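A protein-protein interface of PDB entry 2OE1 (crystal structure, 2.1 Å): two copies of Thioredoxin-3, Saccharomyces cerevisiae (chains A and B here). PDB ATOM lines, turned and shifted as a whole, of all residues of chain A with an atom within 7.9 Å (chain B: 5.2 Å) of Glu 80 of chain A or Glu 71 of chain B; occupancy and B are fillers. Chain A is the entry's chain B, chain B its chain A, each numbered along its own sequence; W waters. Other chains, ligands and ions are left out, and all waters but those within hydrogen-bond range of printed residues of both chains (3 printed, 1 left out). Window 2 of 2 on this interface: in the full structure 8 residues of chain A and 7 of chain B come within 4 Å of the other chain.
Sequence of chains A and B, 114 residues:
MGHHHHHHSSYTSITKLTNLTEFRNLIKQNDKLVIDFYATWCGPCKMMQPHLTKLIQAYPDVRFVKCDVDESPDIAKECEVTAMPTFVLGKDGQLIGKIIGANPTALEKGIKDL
Position printed for both chains: 73.
The side-chain carboxylate (OD1) of Asp 70 of chain B is in salt-bridge range of the side-chain amino group (NZ) of Lys 98 of chain A, at 2.9 Å.
Of the printed residues of chain B, Glu 78 of chain A touches Trp 41 (3.3 Å). Glu 80 of chain A touches just these residues of chain B: Thr 40 (3.9 Å), Asp 70 (3.5 Å) and Glu 71 (3.7 Å). Of the printed residues of chain A, Trp 41 of chain B touches Glu 78, Cys 79 and Lys 98. Of the printed residues of chain A, Asp 70 of chain B touches Glu 80 (3.5 Å) and Lys 98 (2.9 Å). Glu 71 of chain B touches one residue of chain A. The nearest residue of chain B that does not touch Glu 80 of chain A is Trp 41 of chain B (4.1 Å). The nearest residue of chain A that does not touch Glu 71 of chain B is Lys 77 of chain A (5.9 Å). The nearest printed residue of chain A that does not touch Asp 70 of chain B is Cys 79 of chain A (4.6 Å).
Water W2 bridges the backbone carbonyl oxygen of Glu 78 of chain A (2.7 Å) and the side-chain hydroxyl of Thr 40 of chain B (2.8 Å). Water W3 lies within hydrogen-bond range of O of Glu 80 of chain A (2.9 Å) and OD1 of Asp 70 of chain B (3.4 Å). Water W1 lies within hydrogen-bond range of OE2 of Glu 78 of chain A and O of Thr 40 of chain B.
OD1 of Asp 68 of chain B is in hydrogen-bond range of N of Glu 71 of chain B, at 3.2 Å. The side-chain carboxylate (OD1) of Asp 68 of chain B lies within hydrogen-bond range of the backbone NH (N) of Asp 70 of chain B, at 3.0 Å. The backbone carbonyl oxygen (O) of Cys 79 of chain A sits at hydrogen-bond distance from the side-chain amino group (NZ) of Lys 98 of chain A (2.7 Å). NZ of Lys 98 of chain A is in hydrogen-bond range of O of Glu 80 of chain A (3.2 Å). NZ of Lys 77 of chain A lies within salt-bridge range of OE1 of Glu 80 of chain A, at 3.1 Å. The side-chain amino group (NZ) of Lys 16 of chain B lies within salt-bridge range of the side-chain carboxylate (OE1) of Glu 71 of chain B (2.7 Å).
Of the 9 printed residues of chain B, 4 touch a printed residue of chain A. Printed residues of chain B that touch a printed residue of chain A: Thr 40, Trp 41, Asp 70 and Glu 71. Along chain A the printed residues that touch a printed residue of chain B span positions 78 to 98. Among the printed residues, Asp or Glu carboxylates within 4 Å of a Lys or Arg side-chain nitrogen of the other chain: Lys 98 of chain A with Asp 70 of chain B.
Among the printed residues, pairs that only touch across the chains: Glu 78 of chain A with Trp 41 of chain B, Glu 80 of chain A with Asp 70 of chain B, Cys 79 of chain A with Trp 41 of chain B, Glu 80 of chain A with Glu 71 of chain B, Lys 98 of chain A with Trp 41 of chain B and Glu 80 of chain A with Thr 40 of chain B.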
ATOM      1  N   PHE A  37      37.306   9.279 -24.437  1.00  0.00           N
ATOM      2  CA  PHE A  37      37.115   9.242 -25.873  1.00  0.00           C
ATOM      3  C   PHE A  37      38.148  10.172 -26.531  1.00  0.00           C
ATOM      4  O   PHE A  37      38.077  11.405 -26.401  1.00  0.00           O
ATOM      5  CB  PHE A  37      35.699   9.701 -26.235  1.00  0.00           C
ATOM      6  CG  PHE A  37      34.630   8.644 -26.000  1.00  0.00           C
ATOM      7  CD1 PHE A  37      33.796   8.704 -24.855  1.00  0.00           C
ATOM      8  CD2 PHE A  37      34.428   7.616 -26.923  1.00  0.00           C
ATOM      9  CE1 PHE A  37      32.793   7.747 -24.632  1.00  0.00           C
ATOM     10  CE2 PHE A  37      33.404   6.646 -26.699  1.00  0.00           C
ATOM     11  CZ  PHE A  37      32.614   6.710 -25.559  1.00  0.00           C
ATOM     12  N   PRO A  73      33.826   4.188 -34.205  1.00  0.00           N
ATOM     13  CA  PRO A  73      32.899   5.317 -34.422  1.00  0.00           C
ATOM     14  C   PRO A  73      31.495   5.078 -33.886  1.00  0.00           C
ATOM     15  O   PRO A  73      30.773   6.048 -33.598  1.00  0.00           O
ATOM     16  CB  PRO A  73      32.839   5.448 -35.961  1.00  0.00           C
ATOM     17  CG  PRO A  73      33.252   4.092 -36.486  1.00  0.00           C
ATOM     18  CD  PRO A  73      34.292   3.619 -35.487  1.00  0.00           C
ATOM     19  N   ASP A  74      31.081   3.813 -33.796  1.00  0.00           N
ATOM     20  CA  ASP A  74      29.753   3.496 -33.273  1.00  0.00           C
ATOM     21  C   ASP A  74      29.665   3.762 -31.777  1.00  0.00           C
ATOM     22  O   ASP A  74      28.607   4.173 -31.299  1.00  0.00           O
ATOM     23  CB  ASP A  74      29.351   2.044 -33.540  1.00  0.00           C
ATOM     24  CG  ASP A  74      29.319   1.692 -35.033  1.00  0.00           C
ATOM     25  OD1 ASP A  74      29.057   2.584 -35.899  1.00  0.00           O
ATOM     26  OD2 ASP A  74      29.551   0.497 -35.341  1.00  0.00           O
ATOM     27  N   ILE A  75      30.754   3.499 -31.039  1.00  0.00           N
ATOM     28  CA  ILE A  75      30.735   3.767 -29.600  1.00  0.00           C
ATOM     29  C   ILE A  75      30.784   5.294 -29.353  1.00  0.00           C
ATOM     30  O   ILE A  75      30.077   5.809 -28.486  1.00  0.00           O
ATOM     31  CB  ILE A  75      31.858   3.021 -28.810  1.00  0.00           C
ATOM     32  CG1 ILE A  75      31.887   1.526 -29.172  1.00  0.00           C
ATOM     33  CG2 ILE A  75      31.684   3.263 -27.265  1.00  0.00           C
ATOM     34  CD1 ILE A  75      33.086   0.783 -28.581  1.00  0.00           C
ATOM     35  N   ALA A  76      31.637   5.996 -30.102  1.00  0.00           N
ATOM     36  CA  ALA A  76      31.680   7.484 -30.092  1.00  0.00           C
ATOM     37  C   ALA A  76      30.325   8.074 -30.399  1.00  0.00           C
ATOM     38  O   ALA A  76      29.909   9.058 -29.761  1.00  0.00           O
ATOM     39  CB  ALA A  76      32.735   8.018 -31.090  1.00  0.00           C
ATOM     40  N   LYS A  77      29.645   7.485 -31.390  1.00  0.00           N
ATOM     41  CA  LYS A  77      28.330   7.951 -31.829  1.00  0.00           C
ATOM     42  C   LYS A  77      27.273   7.741 -30.741  1.00  0.00           C
ATOM     43  O   LYS A  77      26.417   8.616 -30.504  1.00  0.00           O
ATOM     44  CB  LYS A  77      27.883   7.283 -33.150  1.00  0.00           C
ATOM     45  CG  LYS A  77      26.463   7.649 -33.610  1.00  0.00           C
ATOM     46  CD  LYS A  77      26.247   9.171 -33.599  1.00  0.00           C
ATOM     47  CE  LYS A  77      24.919   9.625 -34.270  1.00  0.00           C
ATOM     48  NZ  LYS A  77      25.082  11.114 -34.556  1.00  0.00           N
ATOM     49  N   GLU A  78      27.339   6.584 -30.092  1.00  0.00           N
ATOM     50  CA  GLU A  78      26.459   6.274 -28.962  1.00  0.00           C
ATOM     51  C   GLU A  78      26.547   7.356 -27.866  1.00  0.00           C
ATOM     52  O   GLU A  78      25.538   7.705 -27.276  1.00  0.00           O
ATOM     53  CB  GLU A  78      26.822   4.903 -28.371  1.00  0.00           C
ATOM     54  CG  GLU A  78      25.924   4.427 -27.248  1.00  0.00           C
ATOM     55  CD  GLU A  78      24.644   3.763 -27.763  1.00  0.00           C
ATOM     56  OE1 GLU A  78      24.599   3.345 -28.941  1.00  0.00           O
ATOM     57  OE2 GLU A  78      23.679   3.636 -26.989  1.00  0.00           O
ATOM     58  N   CYS A  79      27.755   7.860 -27.590  1.00  0.00           N
ATOM     59  CA  CYS A  79      27.965   8.923 -26.585  1.00  0.00           C
ATOM     60  C   CYS A  79      27.966  10.361 -27.138  1.00  0.00           C
ATOM     61  O   CYS A  79      28.392  11.306 -26.447  1.00  0.00           O
ATOM     62  CB  CYS A  79      29.241   8.647 -25.777  1.00  0.00           C
ATOM     63  SG  CYS A  79      29.012   7.205 -24.751  1.00  0.00           S
ATOM     64  N   GLU A  80      27.508  10.491 -28.384  1.00  0.00           N
ATOM     65  CA  GLU A  80      27.479  11.753 -29.143  1.00  0.00           C
ATOM     66  C   GLU A  80      28.790  12.567 -29.062  1.00  0.00           C
ATOM     67  O   GLU A  80      28.787  13.776 -28.792  1.00  0.00           O
ATOM     68  CB  GLU A  80      26.256  12.578 -28.750  1.00  0.00           C
ATOM     69  CG  GLU A  80      24.940  11.950 -29.122  1.00  0.00           C
ATOM     70  CD  GLU A  80      24.548  12.232 -30.573  1.00  0.00           C
ATOM     71  OE1 GLU A  80      25.012  11.496 -31.487  1.00  0.00           O
ATOM     72  OE2 GLU A  80      23.741  13.190 -30.801  1.00  0.00           O
ATOM     73  N   VAL A  81      29.910  11.885 -29.307  1.00  0.00           N
ATOM     74  CA  VAL A  81      31.225  12.510 -29.208  1.00  0.00           C
ATOM     75  C   VAL A  81      31.719  13.082 -30.561  1.00  0.00           C
ATOM     76  O   VAL A  81      32.045  12.335 -31.484  1.00  0.00           O
ATOM     77  CB  VAL A  81      32.292  11.523 -28.608  1.00  0.00           C
ATOM     78  CG1 VAL A  81      33.635  12.200 -28.479  1.00  0.00           C
ATOM     79  CG2 VAL A  81      31.850  10.943 -27.262  1.00  0.00           C
ATOM     80  N   THR A  82      31.810  14.399 -30.680  1.00  0.00           N
ATOM     81  CA  THR A  82      32.443  14.963 -31.892  1.00  0.00           C
ATOM     82  C   THR A  82      33.631  15.927 -31.606  1.00  0.00           C
ATOM     83  O   THR A  82      34.339  16.374 -32.548  1.00  0.00           O
ATOM     84  CB  THR A  82      31.405  15.629 -32.823  1.00  0.00           C
ATOM     85  OG1 THR A  82      30.523  16.430 -32.033  1.00  0.00           O
ATOM     86  CG2 THR A  82      30.588  14.576 -33.571  1.00  0.00           C
ATOM     87  N   ALA A  83      33.816  16.249 -30.320  1.00  0.00           N
ATOM     88  CA  ALA A  83      35.009  16.956 -29.851  1.00  0.00           C
ATOM     89  C   ALA A  83      35.782  16.050 -28.900  1.00  0.00           C
ATOM     90  O   ALA A  83      35.179  15.300 -28.103  1.00  0.00           O
ATOM     91  CB  ALA A  83      34.638  18.294 -29.159  1.00  0.00           C
ATOM     92  N   THR A  86      36.787  13.798 -24.945  1.00  0.00           N
ATOM     93  CA  THR A  86      35.563  13.858 -24.169  1.00  0.00           C
ATOM     94  C   THR A  86      35.605  12.773 -23.098  1.00  0.00           C
ATOM     95  O   THR A  86      35.884  11.608 -23.411  1.00  0.00           O
ATOM     96  CB  THR A  86      34.305  13.645 -25.051  1.00  0.00           C
ATOM     97  OG1 THR A  86      34.109  14.791 -25.903  1.00  0.00           O
ATOM     98  CG2 THR A  86      33.085  13.477 -24.166  1.00  0.00           C
ATOM     99  N   VAL A  88      33.522  10.668 -20.365  1.00  0.00           N
ATOM    100  CA  VAL A  88      32.143  10.291 -20.074  1.00  0.00           C
ATOM    101  C   VAL A  88      32.178   9.591 -18.707  1.00  0.00           C
ATOM    102  O   VAL A  88      33.032   8.739 -18.471  1.00  0.00           O
ATOM    103  CB  VAL A  88      31.538   9.422 -21.250  1.00  0.00           C
ATOM    104  CG1 VAL A  88      30.241   8.799 -20.882  1.00  0.00           C
ATOM    105  CG2 VAL A  88      31.362  10.265 -22.552  1.00  0.00           C
ATOM    106  N   LYS A  98      29.326  14.156 -18.810  1.00  0.00           N
ATOM    107  CA  LYS A  98      30.331  14.299 -19.858  1.00  0.00           C
ATOM    108  C   LYS A  98      31.147  15.556 -19.562  1.00  0.00           C
ATOM    109  O   LYS A  98      30.580  16.592 -19.239  1.00  0.00           O
ATOM    110  CB  LYS A  98      29.574  14.428 -21.195  1.00  0.00           C
ATOM    111  CG  LYS A  98      30.370  14.813 -22.360  1.00  0.00           C
ATOM    112  CD  LYS A  98      29.469  14.967 -23.565  1.00  0.00           C
ATOM    113  CE  LYS A  98      29.175  13.653 -24.207  1.00  0.00           C
ATOM    114  NZ  LYS A  98      28.762  13.864 -25.617  1.00  0.00           N
ATOM    115  N   ILE A 100      33.958  17.829 -21.551  1.00  0.00           N
ATOM    116  CA  ILE A 100      34.489  17.990 -22.912  1.00  0.00           C
ATOM    117  C   ILE A 100      35.766  18.824 -22.896  1.00  0.00           C
ATOM    118  O   ILE A 100      35.790  19.936 -22.348  1.00  0.00           O
ATOM    119  CB  ILE A 100      33.436  18.648 -23.888  1.00  0.00           C
ATOM    120  CG1 ILE A 100      32.167  17.786 -23.962  1.00  0.00           C
ATOM    121  CG2 ILE A 100      34.034  18.911 -25.274  1.00  0.00           C
ATOM    122  CD1 ILE A 100      31.062  18.353 -24.823  1.00  0.00           C
ATOM    123  N   LYS B  16      10.872  18.971 -30.353  1.00  0.00           N
ATOM    124  CA  LYS B  16      12.274  19.019 -30.012  1.00  0.00           C
ATOM    125  C   LYS B  16      12.895  20.299 -30.593  1.00  0.00           C
ATOM    126  O   LYS B  16      12.847  20.527 -31.807  1.00  0.00           O
ATOM    127  CB  LYS B  16      13.019  17.766 -30.479  1.00  0.00           C
ATOM    128  CG  LYS B  16      14.528  17.924 -30.384  1.00  0.00           C
ATOM    129  CD  LYS B  16      15.301  16.637 -30.480  1.00  0.00           C
ATOM    130  CE  LYS B  16      15.296  16.030 -31.822  1.00  0.00           C
ATOM    131  NZ  LYS B  16      16.479  15.159 -31.833  1.00  0.00           N
ATOM    132  N   THR B  40      20.947  11.706 -25.130  1.00  0.00           N
ATOM    133  CA  THR B  40      20.488  10.344 -25.445  1.00  0.00           C
ATOM    134  C   THR B  40      21.269   9.232 -24.727  1.00  0.00           C
ATOM    135  O   THR B  40      20.702   8.196 -24.422  1.00  0.00           O
ATOM    136  CB  THR B  40      20.505  10.067 -26.979  1.00  0.00           C
ATOM    137  OG1 THR B  40      21.810  10.343 -27.491  1.00  0.00           O
ATOM    138  CG2 THR B  40      19.464  10.938 -27.738  1.00  0.00           C
ATOM    139  N   TRP B  41      22.561   9.425 -24.452  1.00  0.00           N
ATOM    140  CA  TRP B  41      23.364   8.375 -23.782  1.00  0.00           C
ATOM    141  C   TRP B  41      23.142   8.377 -22.249  1.00  0.00           C
ATOM    142  O   TRP B  41      23.607   7.478 -21.547  1.00  0.00           O
ATOM    143  CB  TRP B  41      24.855   8.553 -24.118  1.00  0.00           C
ATOM    144  CG  TRP B  41      25.252  10.019 -23.963  1.00  0.00           C
ATOM    145  CD1 TRP B  41      25.276  10.978 -24.950  1.00  0.00           C
ATOM    146  CD2 TRP B  41      25.583  10.700 -22.734  1.00  0.00           C
ATOM    147  NE1 TRP B  41      25.602  12.203 -24.408  1.00  0.00           N
ATOM    148  CE2 TRP B  41      25.794  12.059 -23.055  1.00  0.00           C
ATOM    149  CE3 TRP B  41      25.696  10.294 -21.388  1.00  0.00           C
ATOM    150  CZ2 TRP B  41      26.147  13.001 -22.092  1.00  0.00           C
ATOM    151  CZ3 TRP B  41      26.033  11.241 -20.441  1.00  0.00           C
ATOM    152  CH2 TRP B  41      26.260  12.579 -20.798  1.00  0.00           C
ATOM    153  N   ASP B  68      17.998  18.227 -27.222  1.00  0.00           N
ATOM    154  CA  ASP B  68      19.194  17.361 -27.152  1.00  0.00           C
ATOM    155  C   ASP B  68      20.451  18.243 -27.041  1.00  0.00           C
ATOM    156  O   ASP B  68      20.834  18.908 -28.001  1.00  0.00           O
ATOM    157  CB  ASP B  68      19.218  16.441 -28.372  1.00  0.00           C
ATOM    158  CG  ASP B  68      20.370  15.453 -28.371  1.00  0.00           C
ATOM    159  OD1 ASP B  68      21.478  15.763 -27.911  1.00  0.00           O
ATOM    160  OD2 ASP B  68      20.155  14.332 -28.836  1.00  0.00           O
ATOM    161  N   VAL B  69      21.094  18.229 -25.869  1.00  0.00           N
ATOM    162  CA  VAL B  69      22.243  19.120 -25.614  1.00  0.00           C
ATOM    163  C   VAL B  69      23.481  18.884 -26.515  1.00  0.00           C
ATOM    164  O   VAL B  69      24.250  19.830 -26.747  1.00  0.00           O
ATOM    165  CB  VAL B  69      22.692  19.170 -24.095  1.00  0.00           C
ATOM    166  CG1 VAL B  69      21.528  19.588 -23.145  1.00  0.00           C
ATOM    167  CG2 VAL B  69      23.307  17.845 -23.653  1.00  0.00           C
ATOM    168  N   ASP B  70      23.694  17.643 -26.992  1.00  0.00           N
ATOM    169  CA  ASP B  70      24.793  17.359 -27.944  1.00  0.00           C
ATOM    170  C   ASP B  70      24.442  17.869 -29.352  1.00  0.00           C
ATOM    171  O   ASP B  70      25.323  18.347 -30.087  1.00  0.00           O
ATOM    172  CB  ASP B  70      25.110  15.852 -28.012  1.00  0.00           C
ATOM    173  CG  ASP B  70      25.638  15.301 -26.691  1.00  0.00           C
ATOM    174  OD1 ASP B  70      26.698  15.769 -26.240  1.00  0.00           O
ATOM    175  OD2 ASP B  70      24.988  14.402 -26.095  1.00  0.00           O
ATOM    176  N   GLU B  71      23.170  17.724 -29.741  1.00  0.00           N
ATOM    177  CA  GLU B  71      22.674  18.208 -31.031  1.00  0.00           C
ATOM    178  C   GLU B  71      22.557  19.740 -31.060  1.00  0.00           C
ATOM    179  O   GLU B  71      22.797  20.364 -32.085  1.00  0.00           O
ATOM    180  CB  GLU B  71      21.326  17.543 -31.418  1.00  0.00           C
ATOM    181  CG  GLU B  71      21.498  16.030 -31.742  1.00  0.00           C
ATOM    182  CD  GLU B  71      20.219  15.274 -32.150  1.00  0.00           C
ATOM    183  OE1 GLU B  71      19.079  15.831 -32.070  1.00  0.00           O
ATOM    184  OE2 GLU B  71      20.372  14.088 -32.559  1.00  0.00           O
ATOM    185  N   SER B  72      22.212  20.346 -29.927  1.00  0.00           N
ATOM    186  CA  SER B  72      21.963  21.793 -29.904  1.00  0.00           C
ATOM    187  C   SER B  72      22.745  22.452 -28.789  1.00  0.00           C
ATOM    188  O   SER B  72      22.152  22.990 -27.843  1.00  0.00           O
ATOM    189  CB  SER B  72      20.467  22.017 -29.723  1.00  0.00           C
ATOM    190  OG  SER B  72      19.789  21.409 -30.806  1.00  0.00           O
ATOM    191  N   PRO B  73      24.094  22.427 -28.895  1.00  0.00           N
ATOM    192  CA  PRO B  73      24.817  22.885 -27.734  1.00  0.00           C
ATOM    193  C   PRO B  73      24.709  24.409 -27.542  1.00  0.00           C
ATOM    194  O   PRO B  73      25.002  24.892 -26.442  1.00  0.00           O
ATOM    195  CB  PRO B  73      26.257  22.436 -28.015  1.00  0.00           C
ATOM    196  CG  PRO B  73      26.347  22.436 -29.529  1.00  0.00           C
ATOM    197  CD  PRO B  73      24.985  22.001 -29.999  1.00  0.00           C
HETATM  198  O   HOH W   1      21.764   5.308 -25.547  1.00  0.00           O
HETATM  199  O   HOH W   2      22.892   7.812 -27.779  1.00  0.00           O
HETATM  200  O   HOH W   3      28.674  16.644 -28.925  1.00  0.00           O
